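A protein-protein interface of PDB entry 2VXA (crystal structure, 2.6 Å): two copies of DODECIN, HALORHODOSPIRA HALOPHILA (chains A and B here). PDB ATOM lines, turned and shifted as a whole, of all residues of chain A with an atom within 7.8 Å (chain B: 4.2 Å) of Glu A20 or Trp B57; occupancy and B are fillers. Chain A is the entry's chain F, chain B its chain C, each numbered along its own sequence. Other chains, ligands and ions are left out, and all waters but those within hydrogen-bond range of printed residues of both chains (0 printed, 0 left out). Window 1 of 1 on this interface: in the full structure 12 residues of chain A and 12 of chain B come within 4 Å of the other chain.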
ATOM      1  N   SER A  15     -13.107 -16.005 -13.243  1.00  0.00           N
ATOM      2  CA  SER A  15     -12.856 -15.934 -11.815  1.00  0.00           C
ATOM      3  C   SER A  15     -11.919 -17.048 -11.439  1.00  0.00           C
ATOM      4  O   SER A  15     -12.024 -18.144 -11.968  1.00  0.00           O
ATOM      5  CB  SER A  15     -14.130 -16.017 -11.010  1.00  0.00           C
ATOM      6  OG  SER A  15     -13.848 -16.413  -9.679  1.00  0.00           O
ATOM      7  N   ASN A  17     -12.117 -18.342  -8.650  1.00  0.00           N
ATOM      8  CA  ASN A  17     -12.847 -19.045  -7.586  1.00  0.00           C
ATOM      9  C   ASN A  17     -13.909 -20.056  -7.971  1.00  0.00           C
ATOM     10  O   ASN A  17     -14.184 -20.964  -7.206  1.00  0.00           O
ATOM     11  CB  ASN A  17     -13.502 -18.049  -6.641  1.00  0.00           C
ATOM     12  CG  ASN A  17     -12.500 -17.381  -5.733  1.00  0.00           C
ATOM     13  OD1 ASN A  17     -11.606 -18.033  -5.181  1.00  0.00           O
ATOM     14  ND2 ASN A  17     -12.626 -16.077  -5.592  1.00  0.00           N
ATOM     15  N   GLY A  18     -14.549 -19.885  -9.121  1.00  0.00           N
ATOM     16  CA  GLY A  18     -15.527 -20.868  -9.530  1.00  0.00           C
ATOM     17  C   GLY A  18     -16.576 -20.345 -10.469  1.00  0.00           C
ATOM     18  O   GLY A  18     -16.460 -19.218 -10.981  1.00  0.00           O
ATOM     19  N   ILE A  19     -17.600 -21.169 -10.669  1.00  0.00           N
ATOM     20  CA  ILE A  19     -18.553 -20.940 -11.717  1.00  0.00           C
ATOM     21  C   ILE A  19     -19.461 -19.774 -11.406  1.00  0.00           C
ATOM     22  O   ILE A  19     -19.531 -18.866 -12.214  1.00  0.00           O
ATOM     23  CB  ILE A  19     -19.321 -22.239 -12.096  1.00  0.00           C
ATOM     24  CG1 ILE A  19     -18.339 -23.221 -12.711  1.00  0.00           C
ATOM     25  CG2 ILE A  19     -20.432 -21.945 -13.064  1.00  0.00           C
ATOM     26  CD1 ILE A  19     -18.741 -24.616 -12.556  1.00  0.00           C
ATOM     27  N   GLU A  20     -20.127 -19.802 -10.254  1.00  0.00           N
ATOM     28  CA  GLU A  20     -21.028 -18.736  -9.844  1.00  0.00           C
ATOM     29  C   GLU A  20     -20.345 -17.356  -9.835  1.00  0.00           C
ATOM     30  O   GLU A  20     -20.936 -16.352 -10.246  1.00  0.00           O
ATOM     31  CB  GLU A  20     -21.639 -19.053  -8.481  1.00  0.00           C
ATOM     32  CG  GLU A  20     -22.604 -20.244  -8.493  1.00  0.00           C
ATOM     33  CD  GLU A  20     -21.940 -21.609  -8.175  1.00  0.00           C
ATOM     34  OE1 GLU A  20     -20.710 -21.750  -8.390  1.00  0.00           O
ATOM     35  OE2 GLU A  20     -22.668 -22.539  -7.721  1.00  0.00           O
ATOM     36  N   GLU A  21     -19.093 -17.320  -9.397  1.00  0.00           N
ATOM     37  CA  GLU A  21     -18.331 -16.083  -9.289  1.00  0.00           C
ATOM     38  C   GLU A  21     -18.022 -15.538 -10.673  1.00  0.00           C
ATOM     39  O   GLU A  21     -18.210 -14.336 -10.948  1.00  0.00           O
ATOM     40  CB  GLU A  21     -17.032 -16.294  -8.485  1.00  0.00           C
ATOM     41  CG  GLU A  21     -17.209 -16.781  -7.024  1.00  0.00           C
ATOM     42  CD  GLU A  21     -17.580 -18.291  -6.901  1.00  0.00           C
ATOM     43  OE1 GLU A  21     -17.981 -18.705  -5.796  1.00  0.00           O
ATOM     44  OE2 GLU A  21     -17.477 -19.076  -7.881  1.00  0.00           O
ATOM     45  N   ALA A  22     -17.567 -16.424 -11.550  1.00  0.00           N
ATOM     46  CA  ALA A  22     -17.385 -16.084 -12.967  1.00  0.00           C
ATOM     47  C   ALA A  22     -18.631 -15.481 -13.628  1.00  0.00           C
ATOM     48  O   ALA A  22     -18.515 -14.457 -14.291  1.00  0.00           O
ATOM     49  CB  ALA A  22     -16.916 -17.271 -13.729  1.00  0.00           C
ATOM     50  N   VAL A  23     -19.814 -16.071 -13.436  1.00  0.00           N
ATOM     51  CA  VAL A  23     -20.999 -15.465 -14.075  1.00  0.00           C
ATOM     52  C   VAL A  23     -21.401 -14.150 -13.440  1.00  0.00           C
ATOM     53  O   VAL A  23     -21.725 -13.215 -14.147  1.00  0.00           O
ATOM     54  CB  VAL A  23     -22.203 -16.431 -14.398  1.00  0.00           C
ATOM     55  CG1 VAL A  23     -21.897 -17.838 -13.986  1.00  0.00           C
ATOM     56  CG2 VAL A  23     -23.529 -15.917 -13.842  1.00  0.00           C
ATOM     57  N   ASN A  24     -21.325 -14.074 -12.117  1.00  0.00           N
ATOM     58  CA  ASN A  24     -21.566 -12.804 -11.431  1.00  0.00           C
ATOM     59  C   ASN A  24     -20.661 -11.642 -11.913  1.00  0.00           C
ATOM     60  O   ASN A  24     -21.149 -10.526 -12.150  1.00  0.00           O
ATOM     61  CB  ASN A  24     -21.471 -12.969  -9.931  1.00  0.00           C
ATOM     62  CG  ASN A  24     -22.736 -13.500  -9.339  1.00  0.00           C
ATOM     63  OD1 ASN A  24     -22.682 -14.375  -8.490  1.00  0.00           O
ATOM     64  ND2 ASN A  24     -23.886 -12.981  -9.769  1.00  0.00           N
ATOM     65  N   ASN A  25     -19.370 -11.922 -12.104  1.00  0.00           N
ATOM     66  CA  ASN A  25     -18.495 -10.934 -12.685  1.00  0.00           C
ATOM     67  C   ASN A  25     -18.997 -10.470 -14.039  1.00  0.00           C
ATOM     68  O   ASN A  25     -19.017  -9.261 -14.307  1.00  0.00           O
ATOM     69  CB  ASN A  25     -17.068 -11.439 -12.797  1.00  0.00           C
ATOM     70  CG  ASN A  25     -16.399 -11.635 -11.458  1.00  0.00           C
ATOM     71  OD1 ASN A  25     -15.343 -12.241 -11.382  1.00  0.00           O
ATOM     72  ND2 ASN A  25     -16.988 -11.109 -10.404  1.00  0.00           N
ATOM     73  N   ALA A  26     -19.427 -11.416 -14.877  1.00  0.00           N
ATOM     74  CA  ALA A  26     -19.897 -11.075 -16.219  1.00  0.00           C
ATOM     75  C   ALA A  26     -21.155 -10.226 -16.131  1.00  0.00           C
ATOM     76  O   ALA A  26     -21.291  -9.253 -16.829  1.00  0.00           O
ATOM     77  CB  ALA A  26     -20.141 -12.307 -17.039  1.00  0.00           C
ATOM     78  N   ILE A  27     -22.051 -10.583 -15.242  1.00  0.00           N
ATOM     79  CA  ILE A  27     -23.288  -9.835 -15.064  1.00  0.00           C
ATOM     80  C   ILE A  27     -23.083  -8.459 -14.414  1.00  0.00           C
ATOM     81  O   ILE A  27     -23.714  -7.492 -14.817  1.00  0.00           O
ATOM     82  CB  ILE A  27     -24.335 -10.701 -14.363  1.00  0.00           C
ATOM     83  CG1 ILE A  27     -24.940 -11.612 -15.419  1.00  0.00           C
ATOM     84  CG2 ILE A  27     -25.409  -9.846 -13.743  1.00  0.00           C
ATOM     85  CD1 ILE A  27     -25.426 -12.880 -14.909  1.00  0.00           C
ATOM     86  N   PHE A  40     -30.402 -14.622 -17.938  1.00  0.00           N
ATOM     87  CA  PHE A  40     -29.212 -15.148 -18.585  1.00  0.00           C
ATOM     88  C   PHE A  40     -29.300 -16.639 -18.754  1.00  0.00           C
ATOM     89  O   PHE A  40     -30.138 -17.302 -18.133  1.00  0.00           O
ATOM     90  CB  PHE A  40     -27.965 -14.794 -17.790  1.00  0.00           C
ATOM     91  CG  PHE A  40     -27.791 -15.617 -16.538  1.00  0.00           C
ATOM     92  CD1 PHE A  40     -27.070 -16.793 -16.577  1.00  0.00           C
ATOM     93  CD2 PHE A  40     -28.375 -15.225 -15.337  1.00  0.00           C
ATOM     94  CE1 PHE A  40     -26.943 -17.564 -15.457  1.00  0.00           C
ATOM     95  CE2 PHE A  40     -28.248 -15.977 -14.214  1.00  0.00           C
ATOM     96  CZ  PHE A  40     -27.529 -17.146 -14.250  1.00  0.00           C
ATOM     97  N   VAL A  42     -26.360 -19.966 -19.304  1.00  0.00           N
ATOM     98  CA  VAL A  42     -24.994 -20.425 -19.440  1.00  0.00           C
ATOM     99  C   VAL A  42     -24.836 -21.184 -20.750  1.00  0.00           C
ATOM    100  O   VAL A  42     -25.538 -22.135 -20.996  1.00  0.00           O
ATOM    101  CB  VAL A  42     -24.555 -21.316 -18.265  1.00  0.00           C
ATOM    102  CG1 VAL A  42     -23.201 -21.976 -18.535  1.00  0.00           C
ATOM    103  CG2 VAL A  42     -24.547 -20.532 -16.962  1.00  0.00           C
ATOM    104  N   TRP A  57     -11.616 -19.964 -14.027  1.00  0.00           N
ATOM    105  CA  TRP A  57     -12.889 -20.497 -14.531  1.00  0.00           C
ATOM    106  C   TRP A  57     -13.532 -19.494 -15.502  1.00  0.00           C
ATOM    107  O   TRP A  57     -13.706 -18.319 -15.176  1.00  0.00           O
ATOM    108  CB  TRP A  57     -13.840 -20.746 -13.401  1.00  0.00           C
ATOM    109  CG  TRP A  57     -13.362 -21.720 -12.470  1.00  0.00           C
ATOM    110  CD1 TRP A  57     -12.533 -21.513 -11.405  1.00  0.00           C
ATOM    111  CD2 TRP A  57     -13.684 -23.109 -12.459  1.00  0.00           C
ATOM    112  NE1 TRP A  57     -12.307 -22.694 -10.752  1.00  0.00           N
ATOM    113  CE2 TRP A  57     -13.014 -23.686 -11.374  1.00  0.00           C
ATOM    114  CE3 TRP A  57     -14.489 -23.920 -13.264  1.00  0.00           C
ATOM    115  CZ2 TRP A  57     -13.120 -25.020 -11.073  1.00  0.00           C
ATOM    116  CZ3 TRP A  57     -14.589 -25.243 -12.962  1.00  0.00           C
ATOM    117  CH2 TRP A  57     -13.910 -25.784 -11.890  1.00  0.00           C
ATOM    118  N   VAL A  59     -16.765 -18.819 -17.760  1.00  0.00           N
ATOM    119  CA  VAL A  59     -18.133 -19.207 -18.037  1.00  0.00           C
ATOM    120  C   VAL A  59     -18.712 -18.242 -19.043  1.00  0.00           C
ATOM    121  O   VAL A  59     -18.796 -17.065 -18.797  1.00  0.00           O
ATOM    122  CB  VAL A  59     -19.001 -19.260 -16.754  1.00  0.00           C
ATOM    123  CG1 VAL A  59     -20.370 -19.766 -17.074  1.00  0.00           C
ATOM    124  CG2 VAL A  59     -18.359 -20.179 -15.717  1.00  0.00           C
ATOM    125  N   VAL A  61     -21.805 -16.824 -21.279  1.00  0.00           N
ATOM    126  CA  VAL A  61     -23.124 -16.647 -20.803  1.00  0.00           C
ATOM    127  C   VAL A  61     -23.850 -15.768 -21.814  1.00  0.00           C
ATOM    128  O   VAL A  61     -23.252 -14.915 -22.460  1.00  0.00           O
ATOM    129  CB  VAL A  61     -23.061 -16.037 -19.379  1.00  0.00           C
ATOM    130  CG1 VAL A  61     -23.192 -14.540 -19.427  1.00  0.00           C
ATOM    131  CG2 VAL A  61     -24.135 -16.602 -18.501  1.00  0.00           C
ATOM    132  N   GLY B  13     -34.639 -26.834 -10.914  1.00  0.00           N
ATOM    133  CA  GLY B  13     -34.529 -26.368  -9.553  1.00  0.00           C
ATOM    134  C   GLY B  13     -34.041 -24.941  -9.478  1.00  0.00           C
ATOM    135  O   GLY B  13     -33.303 -24.481 -10.307  1.00  0.00           O
ATOM    136  N   SER B  14     -34.445 -24.268  -8.422  1.00  0.00           N
ATOM    137  CA  SER B  14     -34.145 -22.870  -8.191  1.00  0.00           C
ATOM    138  C   SER B  14     -33.412 -22.664  -6.874  1.00  0.00           C
ATOM    139  O   SER B  14     -33.666 -23.362  -5.893  1.00  0.00           O
ATOM    140  CB  SER B  14     -35.451 -22.114  -8.156  1.00  0.00           C
ATOM    141  OG  SER B  14     -35.239 -20.786  -8.473  1.00  0.00           O
ATOM    142  N   SER B  15     -32.498 -21.705  -6.851  1.00  0.00           N
ATOM    143  CA  SER B  15     -31.808 -21.315  -5.629  1.00  0.00           C
ATOM    144  C   SER B  15     -31.190 -19.930  -5.750  1.00  0.00           C
ATOM    145  O   SER B  15     -30.618 -19.581  -6.775  1.00  0.00           O
ATOM    146  CB  SER B  15     -30.740 -22.332  -5.263  1.00  0.00           C
ATOM    147  OG  SER B  15     -29.826 -21.801  -4.329  1.00  0.00           O
ATOM    148  N   PRO B  16     -31.299 -19.127  -4.692  1.00  0.00           N
ATOM    149  CA  PRO B  16     -30.598 -17.844  -4.718  1.00  0.00           C
ATOM    150  C   PRO B  16     -29.091 -17.992  -4.460  1.00  0.00           C
ATOM    151  O   PRO B  16     -28.346 -17.022  -4.569  1.00  0.00           O
ATOM    152  CB  PRO B  16     -31.273 -17.072  -3.595  1.00  0.00           C
ATOM    153  CG  PRO B  16     -31.719 -18.106  -2.649  1.00  0.00           C
ATOM    154  CD  PRO B  16     -32.069 -19.320  -3.453  1.00  0.00           C
ATOM    155  N   ASN B  17     -28.647 -19.214  -4.161  1.00  0.00           N
ATOM    156  CA  ASN B  17     -27.269 -19.455  -3.776  1.00  0.00           C
ATOM    157  C   ASN B  17     -26.326 -20.012  -4.811  1.00  0.00           C
ATOM    158  O   ASN B  17     -25.139 -19.765  -4.711  1.00  0.00           O
ATOM    159  CB  ASN B  17     -27.215 -20.345  -2.543  1.00  0.00           C
ATOM    160  CG  ASN B  17     -27.635 -19.610  -1.278  1.00  0.00           C
ATOM    161  OD1 ASN B  17     -27.191 -18.476  -0.998  1.00  0.00           O
ATOM    162  ND2 ASN B  17     -28.498 -20.245  -0.511  1.00  0.00           N
ATOM    163  N   GLY B  18     -26.827 -20.777  -5.777  1.00  0.00           N
ATOM    164  CA  GLY B  18     -25.945 -21.330  -6.812  1.00  0.00           C
ATOM    165  C   GLY B  18     -26.368 -22.626  -7.450  1.00  0.00           C
ATOM    166  O   GLY B  18     -27.477 -23.118  -7.236  1.00  0.00           O
ATOM    167  N   ILE B  19     -25.448 -23.206  -8.207  1.00  0.00           N
ATOM    168  CA  ILE B  19     -25.784 -24.339  -9.067  1.00  0.00           C
ATOM    169  C   ILE B  19     -26.083 -25.622  -8.277  1.00  0.00           C
ATOM    170  O   ILE B  19     -27.113 -26.239  -8.469  1.00  0.00           O
ATOM    171  CB  ILE B  19     -24.736 -24.514 -10.194  1.00  0.00           C
ATOM    172  CG1 ILE B  19     -24.798 -23.301 -11.109  1.00  0.00           C
ATOM    173  CG2 ILE B  19     -25.012 -25.749 -11.023  1.00  0.00           C
ATOM    174  CD1 ILE B  19     -23.558 -23.040 -11.831  1.00  0.00           C
ATOM    175  N   GLU B  20     -25.198 -25.982  -7.364  1.00  0.00           N
ATOM    176  CA  GLU B  20     -25.365 -27.221  -6.598  1.00  0.00           C
ATOM    177  C   GLU B  20     -26.611 -27.213  -5.699  1.00  0.00           C
ATOM    178  O   GLU B  20     -27.291 -28.227  -5.538  1.00  0.00           O
ATOM    179  CB  GLU B  20     -24.111 -27.544  -5.767  1.00  0.00           C
ATOM    180  CG  GLU B  20     -22.858 -27.863  -6.571  1.00  0.00           C
ATOM    181  CD  GLU B  20     -22.009 -26.639  -6.931  1.00  0.00           C
ATOM    182  OE1 GLU B  20     -22.550 -25.502  -7.036  1.00  0.00           O
ATOM    183  OE2 GLU B  20     -20.784 -26.829  -7.120  1.00  0.00           O
ATOM    184  N   ALA B  22     -29.320 -25.408  -6.364  1.00  0.00           N
ATOM    185  CA  ALA B  22     -30.461 -25.480  -7.280  1.00  0.00           C
ATOM    186  C   ALA B  22     -30.770 -26.903  -7.712  1.00  0.00           C
ATOM    187  O   ALA B  22     -31.943 -27.286  -7.776  1.00  0.00           O
ATOM    188  CB  ALA B  22     -30.245 -24.603  -8.486  1.00  0.00           C
ATOM    189  N   ARG B  46     -29.519 -21.521 -16.198  1.00  0.00           N
ATOM    190  CA  ARG B  46     -30.125 -20.233 -16.529  1.00  0.00           C
ATOM    191  C   ARG B  46     -30.319 -19.432 -15.248  1.00  0.00           C
ATOM    192  O   ARG B  46     -30.055 -19.906 -14.149  1.00  0.00           O
ATOM    193  CB  ARG B  46     -31.478 -20.400 -17.284  1.00  0.00           C
ATOM    194  CG  ARG B  46     -31.416 -21.277 -18.567  1.00  0.00           C
ATOM    195  CD  ARG B  46     -32.778 -21.665 -19.182  1.00  0.00           C
ATOM    196  NE  ARG B  46     -33.449 -20.471 -19.660  1.00  0.00           N
ATOM    197  CZ  ARG B  46     -33.265 -19.902 -20.853  1.00  0.00           C
ATOM    198  NH1 ARG B  46     -32.467 -20.430 -21.777  1.00  0.00           N
ATOM    199  NH2 ARG B  46     -33.912 -18.786 -21.115  1.00  0.00           N
ATOM    200  N   VAL B  54     -27.583 -11.606 -10.070  1.00  0.00           N
ATOM    201  CA  VAL B  54     -28.338 -12.838 -10.166  1.00  0.00           C
ATOM    202  C   VAL B  54     -29.101 -13.042  -8.869  1.00  0.00           C
ATOM    203  O   VAL B  54     -28.501 -13.122  -7.815  1.00  0.00           O
ATOM    204  CB  VAL B  54     -27.414 -14.053 -10.390  1.00  0.00           C
ATOM    205  CG1 VAL B  54     -28.227 -15.335 -10.586  1.00  0.00           C
ATOM    206  CG2 VAL B  54     -26.495 -13.827 -11.574  1.00  0.00           C
ATOM    207  N   HIS B  56     -31.811 -15.578  -8.862  1.00  0.00           N
ATOM    208  CA  HIS B  56     -32.220 -16.995  -8.936  1.00  0.00           C
ATOM    209  C   HIS B  56     -31.342 -17.776  -9.907  1.00  0.00           C
ATOM    210  O   HIS B  56     -31.260 -17.426 -11.058  1.00  0.00           O
ATOM    211  CB  HIS B  56     -33.669 -17.143  -9.392  1.00  0.00           C
ATOM    212  CG  HIS B  56     -34.670 -16.542  -8.457  1.00  0.00           C
ATOM    213  ND1 HIS B  56     -35.414 -15.428  -8.779  1.00  0.00           N
ATOM    214  CD2 HIS B  56     -35.045 -16.894  -7.207  1.00  0.00           C
ATOM    215  CE1 HIS B  56     -36.209 -15.125  -7.771  1.00  0.00           C
ATOM    216  NE2 HIS B  56     -35.997 -15.995  -6.803  1.00  0.00           N
ATOM    217  N   TRP B  57     -30.669 -18.820  -9.429  1.00  0.00           N
ATOM    218  CA  TRP B  57     -30.008 -19.785 -10.312  1.00  0.00           C
ATOM    219  C   TRP B  57     -30.999 -20.873 -10.681  1.00  0.00           C
ATOM    220  O   TRP B  57     -31.615 -21.440  -9.811  1.00  0.00           O
ATOM    221  CB  TRP B  57     -28.819 -20.406  -9.620  1.00  0.00           C
ATOM    222  CG  TRP B  57     -27.774 -19.423  -9.325  1.00  0.00           C
ATOM    223  CD1 TRP B  57     -27.702 -18.611  -8.243  1.00  0.00           C
ATOM    224  CD2 TRP B  57     -26.630 -19.122 -10.130  1.00  0.00           C
ATOM    225  NE1 TRP B  57     -26.590 -17.826  -8.320  1.00  0.00           N
ATOM    226  CE2 TRP B  57     -25.921 -18.108  -9.479  1.00  0.00           C
ATOM    227  CE3 TRP B  57     -26.151 -19.605 -11.352  1.00  0.00           C
ATOM    228  CZ2 TRP B  57     -24.767 -17.565  -9.995  1.00  0.00           C
ATOM    229  CZ3 TRP B  57     -25.007 -19.074 -11.861  1.00  0.00           C
ATOM    230  CH2 TRP B  57     -24.320 -18.068 -11.186  1.00  0.00           C
ATOM    231  N   GLN B  58     -31.172 -21.134 -11.970  1.00  0.00           N
ATOM    232  CA  GLN B  58     -32.186 -22.069 -12.409  1.00  0.00           C
ATOM    233  C   GLN B  58     -31.538 -23.183 -13.195  1.00  0.00           C
ATOM    234  O   GLN B  58     -31.145 -23.005 -14.324  1.00  0.00           O
ATOM    235  CB  GLN B  58     -33.269 -21.360 -13.210  1.00  0.00           C
ATOM    236  CG  GLN B  58     -33.938 -20.240 -12.419  1.00  0.00           C
ATOM    237  CD  GLN B  58     -34.470 -19.101 -13.291  1.00  0.00           C
ATOM    238  OE1 GLN B  58     -33.953 -18.822 -14.380  1.00  0.00           O
ATOM    239  NE2 GLN B  58     -35.507 -18.451 -12.815  1.00  0.00           N
ATOM    240  N   VAL B  59     -31.371 -24.330 -12.561  1.00  0.00           N
ATOM    241  CA  VAL B  59     -30.720 -25.448 -13.217  1.00  0.00           C
ATOM    242  C   VAL B  59     -31.750 -26.477 -13.649  1.00  0.00           C
ATOM    243  O   VAL B  59     -32.504 -27.008 -12.855  1.00  0.00           O
ATOM    244  CB  VAL B  59     -29.643 -26.087 -12.374  1.00  0.00           C
ATOM    245  CG1 VAL B  59     -28.927 -27.118 -13.205  1.00  0.00           C
ATOM    246  CG2 VAL B  59     -28.633 -25.025 -11.883  1.00  0.00           C
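The backbone NH of Ile B19 sits at hydrogen-bond distance from the side-chain carboxylate of Glu A20. OE2 of Glu A20 sits close to OE1 of Glu B20.
Glu A20 touches Gly B18, but with the chains exchanged Gly A18 does not touch Glu B20 (8.3 Å). Glu A20 touches Ile B19, but with the chains exchanged Ile A19 does not touch Glu B20 (6.2 Å). Glu A20 touches its own counterpart, Glu B20. Glu A20 touches Trp B57, but with the chains exchanged Trp A57 does not touch Glu B20 (8.4 Å). Positions printed for both chains: 15, 17, 18, 19, 20, 22, 57 and 59. Of the 11 pairs that touch across the chains among the printed residues, 2 have their exchanged pair printed and touching as well.
Of the 15 printed residues of chain B, 6 touch a printed residue of chain A. Hydrophobic or aromatic side chains of chain B that line the printed part of chain A: Ile B19, Val B54 and Trp B57. Of the 17 printed residues of chain A, 6 touch a printed residue of chain B.
Among the printed residues, pairs that only touch across the chains: Ile A19 with Ile B19 (3.5 Å), Glu A20 with Gly B18 (3.6 Å), Glu A20 with Trp B57 (3.6 Å), Val A23 with Trp B57 (3.5 Å), Asn A24 with Val B54 (3.3 Å), Ile A27 with Val B54 (3.6 Å), Phe A40 with Arg B46 (3.3 Å), Phe A40 with Val B54 (3.7 Å) and Phe A40 with Trp B57 (3.97 Å).
The backbone NH (N) of Gly B18 is in hydrogen-bond range of the side-chain hydroxyl (OG) of Ser B15, 3.5 Å away. The backbone carbonyl oxygen (O) of Ser B15 lies within hydrogen-bond range of the backbone NH (N) of Trp B57, at 2.8 Å. The backbone NH of Gln B58 is in hydrogen-bond range of the backbone carbonyl oxygen of Arg B46 (2.7 Å). N of Ile A19 is in hydrogen-bond range of OE2 of Glu A21 (3.5 Å). O of Glu A20 sits close to OD1 of Asn A24, at 3.2 Å.
Glu A20 touches just these residues of chain B: Gly B18 (3.6 Å), Ile B19 (2.9 Å), Glu B20 (3.0 Å) and Trp B57 (3.6 Å). Of chain A, only Glu A20 (3.6 Å), Val A23 (3.5 Å) and Phe A40 (3.97 Å) come within 4 Å of Trp B57. Of the printed residues of chain B, Val A23 touches Trp B57 (3.5 Å). Of the printed residues of chain A, Arg B46 touches Phe A40 (3.3 Å). Printed residues of chain A within 4 Å of Ile B19: Ile A19 and Glu A20. Of the printed residues of chain B, Ile A27 touches Val B54 (3.6 Å). Of the printed residues of chain A, Glu B20 touches Glu A20. The nearest printed residue of chain B that does not touch Glu A20 is Asn B17 (4.6 Å). The nearest residue of chain A that does not touch Trp B57 is Asn A24 (4.1 Å). The nearest printed residue of chain A that does not touch Ile B19 is Val A42 (5.8 Å).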
